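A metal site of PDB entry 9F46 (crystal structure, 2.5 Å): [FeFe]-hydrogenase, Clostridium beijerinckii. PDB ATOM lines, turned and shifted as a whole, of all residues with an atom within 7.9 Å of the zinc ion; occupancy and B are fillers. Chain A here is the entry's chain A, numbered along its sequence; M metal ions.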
ATOM      1  N   ASP A 112       1.264 -11.256   9.064  1.00  0.00           N
ATOM      2  CA  ASP A 112       2.143 -12.340   8.643  1.00  0.00           C
ATOM      3  C   ASP A 112       2.439 -13.239   9.838  1.00  0.00           C
ATOM      4  O   ASP A 112       2.795 -12.753  10.916  1.00  0.00           O
ATOM      5  CB  ASP A 112       3.450 -11.811   8.072  1.00  0.00           C
ATOM      6  CG  ASP A 112       3.269 -11.065   6.774  1.00  0.00           C
ATOM      7  OD1 ASP A 112       3.103 -11.736   5.727  1.00  0.00           O
ATOM      8  OD2 ASP A 112       3.281  -9.819   6.816  1.00  0.00           O
ATOM      9  N   CYS A 113       2.310 -14.554   9.641  1.00  0.00           N
ATOM     10  CA  CYS A 113       2.653 -15.505  10.684  1.00  0.00           C
ATOM     11  C   CYS A 113       4.170 -15.669  10.745  1.00  0.00           C
ATOM     12  O   CYS A 113       4.833 -15.834   9.717  1.00  0.00           O
ATOM     13  CB  CYS A 113       1.993 -16.852  10.416  1.00  0.00           C
ATOM     14  SG  CYS A 113       2.813 -18.256  11.217  1.00  0.00           S
ATOM     15  N   ILE A 114       4.722 -15.619  11.959  1.00  0.00           N
ATOM     16  CA  ILE A 114       6.166 -15.724  12.127  1.00  0.00           C
ATOM     17  C   ILE A 114       6.639 -17.143  11.828  1.00  0.00           C
ATOM     18  O   ILE A 114       7.740 -17.339  11.295  1.00  0.00           O
ATOM     19  CB  ILE A 114       6.573 -15.274  13.543  1.00  0.00           C
ATOM     20  CG1 ILE A 114       8.080 -15.004  13.603  1.00  0.00           C
ATOM     21  CG2 ILE A 114       6.173 -16.324  14.575  1.00  0.00           C
ATOM     22  CD1 ILE A 114       8.509 -13.801  12.782  1.00  0.00           C
ATOM     23  N   ILE A 115       5.831 -18.159  12.141  1.00  0.00           N
ATOM     24  CA  ILE A 115       6.209 -19.537  11.862  1.00  0.00           C
ATOM     25  C   ILE A 115       6.390 -19.754  10.363  1.00  0.00           C
ATOM     26  O   ILE A 115       7.387 -20.316   9.909  1.00  0.00           O
ATOM     27  CB  ILE A 115       5.167 -20.512  12.438  1.00  0.00           C
ATOM     28  CG1 ILE A 115       4.998 -20.305  13.944  1.00  0.00           C
ATOM     29  CG2 ILE A 115       5.559 -21.955  12.128  1.00  0.00           C
ATOM     30  CD1 ILE A 115       6.225 -20.661  14.766  1.00  0.00           C
ATOM     31  N   GLN A 116       5.409 -19.325   9.574  1.00  0.00           N
ATOM     32  CA  GLN A 116       5.494 -19.517   8.129  1.00  0.00           C
ATOM     33  C   GLN A 116       6.703 -18.777   7.565  1.00  0.00           C
ATOM     34  O   GLN A 116       7.450 -19.321   6.731  1.00  0.00           O
ATOM     35  CB  GLN A 116       4.214 -19.031   7.443  1.00  0.00           C
ATOM     36  CG  GLN A 116       2.964 -19.842   7.794  1.00  0.00           C
ATOM     37  CD  GLN A 116       2.984 -21.235   7.198  1.00  0.00           C
ATOM     38  OE1 GLN A 116       3.237 -21.413   6.011  1.00  0.00           O
ATOM     39  NE2 GLN A 116       2.709 -22.239   8.021  1.00  0.00           N
ATOM     40  N   PHE A 117       6.917 -17.543   8.004  1.00  0.00           N
ATOM     41  CA  PHE A 117       8.043 -16.783   7.468  1.00  0.00           C
ATOM     42  C   PHE A 117       9.362 -17.443   7.813  1.00  0.00           C
ATOM     43  O   PHE A 117      10.271 -17.485   6.985  1.00  0.00           O
ATOM     44  CB  PHE A 117       8.056 -15.360   7.996  1.00  0.00           C
ATOM     45  CG  PHE A 117       9.273 -14.595   7.566  1.00  0.00           C
ATOM     46  CD1 PHE A 117       9.353 -14.059   6.298  1.00  0.00           C
ATOM     47  CD2 PHE A 117      10.351 -14.449   8.422  1.00  0.00           C
ATOM     48  CE1 PHE A 117      10.471 -13.365   5.888  1.00  0.00           C
ATOM     49  CE2 PHE A 117      11.482 -13.754   8.018  1.00  0.00           C
ATOM     50  CZ  PHE A 117      11.539 -13.217   6.747  1.00  0.00           C
ATOM     51  N   LYS A 119       9.876 -20.624   8.477  1.00  0.00           N
ATOM     52  CA  LYS A 119      10.002 -21.804   7.622  1.00  0.00           C
ATOM     53  C   LYS A 119      10.592 -21.412   6.276  1.00  0.00           C
ATOM     54  O   LYS A 119      11.517 -22.055   5.770  1.00  0.00           O
ATOM     55  CB  LYS A 119       8.644 -22.475   7.434  1.00  0.00           C
ATOM     56  CG  LYS A 119       8.214 -23.389   8.573  1.00  0.00           C
ATOM     57  CD  LYS A 119       6.783 -23.883   8.386  1.00  0.00           C
ATOM     58  CE  LYS A 119       6.709 -25.032   7.377  1.00  0.00           C
ATOM     59  NZ  LYS A 119       5.311 -25.509   7.188  1.00  0.00           N
ATOM     60  N   ILE A 154       5.293 -27.386  14.083  1.00  0.00           N
ATOM     61  CA  ILE A 154       4.466 -26.365  14.704  1.00  0.00           C
ATOM     62  C   ILE A 154       3.345 -25.941  13.763  1.00  0.00           C
ATOM     63  O   ILE A 154       2.204 -25.744  14.182  1.00  0.00           O
ATOM     64  CB  ILE A 154       5.329 -25.167  15.145  1.00  0.00           C
ATOM     65  CG1 ILE A 154       6.184 -25.558  16.350  1.00  0.00           C
ATOM     66  CG2 ILE A 154       4.459 -23.971  15.490  1.00  0.00           C
ATOM     67  CD1 ILE A 154       7.374 -24.644  16.579  1.00  0.00           C
ATOM     68  N   SER A 155       3.657 -25.792  12.474  1.00  0.00           N
ATOM     69  CA  SER A 155       2.656 -25.339  11.530  1.00  0.00           C
ATOM     70  C   SER A 155       1.584 -26.395  11.292  1.00  0.00           C
ATOM     71  O   SER A 155       0.462 -26.040  10.891  1.00  0.00           O
ATOM     72  CB  SER A 155       3.305 -24.960  10.207  1.00  0.00           C
ATOM     73  OG  SER A 155       3.600 -26.115   9.428  1.00  0.00           O
ATOM     74  N   GLU A 195       3.263 -15.704  20.275  1.00  0.00           N
ATOM     75  CA  GLU A 195       2.719 -16.281  19.058  1.00  0.00           C
ATOM     76  C   GLU A 195       3.075 -17.760  18.934  1.00  0.00           C
ATOM     77  O   GLU A 195       2.230 -18.589  18.562  1.00  0.00           O
ATOM     78  CB  GLU A 195       3.217 -15.514  17.832  1.00  0.00           C
ATOM     79  CG  GLU A 195       2.581 -15.953  16.520  1.00  0.00           C
ATOM     80  CD  GLU A 195       3.068 -15.140  15.337  1.00  0.00           C
ATOM     81  OE1 GLU A 195       3.839 -14.183  15.543  1.00  0.00           O
ATOM     82  OE2 GLU A 195       2.678 -15.460  14.192  1.00  0.00           O
ATOM     83  N   HIS A 199       0.482 -20.915  18.803  1.00  0.00           N
ATOM     84  CA  HIS A 199       0.462 -21.959  17.787  1.00  0.00           C
ATOM     85  C   HIS A 199       0.449 -23.339  18.429  1.00  0.00           C
ATOM     86  O   HIS A 199      -0.309 -24.230  18.020  1.00  0.00           O
ATOM     87  CB  HIS A 199       1.668 -21.826  16.858  1.00  0.00           C
ATOM     88  CG  HIS A 199       1.476 -20.835  15.746  1.00  0.00           C
ATOM     89  ND1 HIS A 199       1.342 -19.485  15.971  1.00  0.00           N
ATOM     90  CD2 HIS A 199       1.410 -21.013  14.409  1.00  0.00           C
ATOM     91  CE1 HIS A 199       1.206 -18.867  14.817  1.00  0.00           C
ATOM     92  NE2 HIS A 199       1.234 -19.768  13.857  1.00  0.00           N
ATOM     93  N   LYS A 204      -3.477 -22.426  17.260  1.00  0.00           N
ATOM     94  CA  LYS A 204      -4.080 -21.262  16.646  1.00  0.00           C
ATOM     95  C   LYS A 204      -2.994 -20.387  16.019  1.00  0.00           C
ATOM     96  O   LYS A 204      -2.004 -20.044  16.677  1.00  0.00           O
ATOM     97  CB  LYS A 204      -4.887 -20.459  17.672  1.00  0.00           C
ATOM     98  CG  LYS A 204      -4.937 -18.965  17.449  1.00  0.00           C
ATOM     99  CD  LYS A 204      -6.047 -18.320  18.279  1.00  0.00           C
ATOM    100  CE  LYS A 204      -5.495 -17.330  19.309  1.00  0.00           C
ATOM    101  NZ  LYS A 204      -5.021 -16.082  18.660  1.00  0.00           N
ATOM    102  N   CYS A 205      -3.200 -20.028  14.762  1.00  0.00           N
ATOM    103  CA  CYS A 205      -2.344 -19.117  14.013  1.00  0.00           C
ATOM    104  C   CYS A 205      -3.142 -17.836  13.834  1.00  0.00           C
ATOM    105  O   CYS A 205      -4.049 -17.773  12.995  1.00  0.00           O
ATOM    106  CB  CYS A 205      -1.930 -19.749  12.688  1.00  0.00           C
ATOM    107  SG  CYS A 205      -0.968 -18.689  11.643  1.00  0.00           S
ATOM    108  N   TYR A 206      -2.819 -16.814  14.624  1.00  0.00           N
ATOM    109  CA  TYR A 206      -3.686 -15.638  14.713  1.00  0.00           C
ATOM    110  C   TYR A 206      -3.778 -14.892  13.394  1.00  0.00           C
ATOM    111  O   TYR A 206      -4.748 -14.144  13.193  1.00  0.00           O
ATOM    112  CB  TYR A 206      -3.220 -14.719  15.855  1.00  0.00           C
ATOM    113  CG  TYR A 206      -2.141 -13.722  15.498  1.00  0.00           C
ATOM    114  CD1 TYR A 206      -0.799 -14.045  15.636  1.00  0.00           C
ATOM    115  CD2 TYR A 206      -2.467 -12.442  15.052  1.00  0.00           C
ATOM    116  CE1 TYR A 206       0.201 -13.126  15.325  1.00  0.00           C
ATOM    117  CE2 TYR A 206      -1.480 -11.523  14.735  1.00  0.00           C
ATOM    118  CZ  TYR A 206      -0.153 -11.875  14.869  1.00  0.00           C
ATOM    119  OH  TYR A 206       0.824 -10.954  14.556  1.00  0.00           O
ATOM    120  N   THR A 207      -2.819 -15.069  12.484  1.00  0.00           N
ATOM    121  CA  THR A 207      -2.917 -14.495  11.149  1.00  0.00           C
ATOM    122  C   THR A 207      -3.518 -15.460  10.124  1.00  0.00           C
ATOM    123  O   THR A 207      -3.799 -15.039   8.996  1.00  0.00           O
ATOM    124  CB  THR A 207      -1.540 -14.045  10.655  1.00  0.00           C
ATOM    125  OG1 THR A 207      -0.736 -15.199  10.352  1.00  0.00           O
ATOM    126  CG2 THR A 207      -0.836 -13.216  11.718  1.00  0.00           C
ATOM    127  N   SER A 208      -3.713 -16.725  10.481  1.00  0.00           N
ATOM    128  CA  SER A 208      -4.334 -17.729   9.626  1.00  0.00           C
ATOM    129  C   SER A 208      -3.535 -18.043   8.370  1.00  0.00           C
ATOM    130  O   SER A 208      -4.111 -18.490   7.379  1.00  0.00           O
ATOM    131  CB  SER A 208      -5.753 -17.298   9.231  1.00  0.00           C
ATOM    132  OG  SER A 208      -6.527 -16.970  10.370  1.00  0.00           O
ATOM    133  N   GLN A 209      -2.220 -17.831   8.388  1.00  0.00           N
ATOM    134  CA  GLN A 209      -1.373 -18.234   7.271  1.00  0.00           C
ATOM    135  C   GLN A 209      -1.024 -19.724   7.311  1.00  0.00           C
ATOM    136  O   GLN A 209      -0.673 -20.298   6.270  1.00  0.00           O
ATOM    137  CB  GLN A 209      -0.090 -17.408   7.249  1.00  0.00           C
ATOM    138  CG  GLN A 209      -0.310 -15.912   7.088  1.00  0.00           C
ATOM    139  CD  GLN A 209       0.922 -15.193   6.538  1.00  0.00           C
ATOM    140  OE1 GLN A 209       2.002 -15.261   7.112  1.00  0.00           O
ATOM    141  NE2 GLN A 209       0.751 -14.508   5.412  1.00  0.00           N
ATOM    142  N   CYS A 210      -1.095 -20.352   8.487  1.00  0.00           N
ATOM    143  CA  CYS A 210      -0.849 -21.793   8.613  1.00  0.00           C
ATOM    144  C   CYS A 210      -2.130 -22.526   8.211  1.00  0.00           C
ATOM    145  O   CYS A 210      -3.051 -22.678   9.016  1.00  0.00           O
ATOM    146  CB  CYS A 210      -0.453 -22.148  10.046  1.00  0.00           C
ATOM    147  SG  CYS A 210       1.210 -21.677  10.567  1.00  0.00           S
ATOM    148  N   ASN A 211      -2.183 -22.998   6.957  1.00  0.00           N
ATOM    149  CA  ASN A 211      -3.420 -23.567   6.439  1.00  0.00           C
ATOM    150  C   ASN A 211      -3.892 -24.779   7.234  1.00  0.00           C
ATOM    151  O   ASN A 211      -5.076 -25.127   7.180  1.00  0.00           O
ATOM    152  CB  ASN A 211      -3.259 -23.950   4.972  1.00  0.00           C
ATOM    153  CG  ASN A 211      -2.001 -24.756   4.711  1.00  0.00           C
ATOM    154  OD1 ASN A 211      -0.908 -24.359   5.124  1.00  0.00           O
ATOM    155  ND2 ASN A 211      -2.148 -25.891   4.036  1.00  0.00           N
ATOM    156  N   LEU A 213      -3.927 -25.042  10.470  1.00  0.00           N
ATOM    157  CA  LEU A 213      -4.583 -24.613  11.696  1.00  0.00           C
ATOM    158  C   LEU A 213      -5.827 -23.768  11.437  1.00  0.00           C
ATOM    159  O   LEU A 213      -6.469 -23.339  12.403  1.00  0.00           O
ATOM    160  CB  LEU A 213      -3.600 -23.821  12.565  1.00  0.00           C
ATOM    161  CG  LEU A 213      -2.299 -24.547  12.943  1.00  0.00           C
ATOM    162  CD1 LEU A 213      -1.392 -23.632  13.765  1.00  0.00           C
ATOM    163  CD2 LEU A 213      -2.599 -25.828  13.702  1.00  0.00           C
ATOM    164  N   VAL A 214      -6.182 -23.516  10.190  1.00  0.00           N
ATOM    165  CA  VAL A 214      -7.342 -22.684   9.870  1.00  0.00           C
ATOM    166  C   VAL A 214      -8.567 -23.586   9.717  1.00  0.00           C
ATOM    167  O   VAL A 214      -8.506 -24.636   9.056  1.00  0.00           O
ATOM    168  CB  VAL A 214      -7.113 -21.861   8.588  1.00  0.00           C
ATOM    169  CG1 VAL A 214      -5.919 -20.924   8.760  1.00  0.00           C
ATOM    170  CG2 VAL A 214      -6.920 -22.783   7.377  1.00  0.00           C
HETATM  171 ZN    ZN M   1       1.095 -19.691  11.767  1.00  0.00          ZN
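O of Glu 195 lies within hydrogen-bond range of ND1 of His 199 (2.9 Å). The backbone carbonyl oxygen (O) of Lys 204 sits close to the backbone NH (N) of His 199. The side-chain sulfur of Cys 205 lies close to the side-chain hydroxyl of Thr 207, at 3.7 Å. SG of Cys 205 lies close to N of Ser 208, 3.6 Å away. SG of Cys 113 lies close to N of Ile 115 (3.2 Å). N of Gln 116 sits close to SG of Cys 113, 3.3 Å away. OE1 of Gln 209 lies within hydrogen-bond range of N of Cys 113, at 2.6 Å. The side-chain hydroxyl (OG1) of Thr 207 sits close to the backbone NH (N) of Cys 113 (3.2 Å).
Four residues have an atom within 4 Å of the zinc ion: Cys 113, His 199, Cys 205 and Cys 210. The nearest printed residue that does not touch the zinc ion is Ile 115 (4.2 Å).
The zinc ion is bound by NE2 of His 199 (2.1 Å), SG of Cys 205 (2.3 Å), SG of Cys 113 (2.3 Å) and SG of Cys 210 (2.3 Å).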
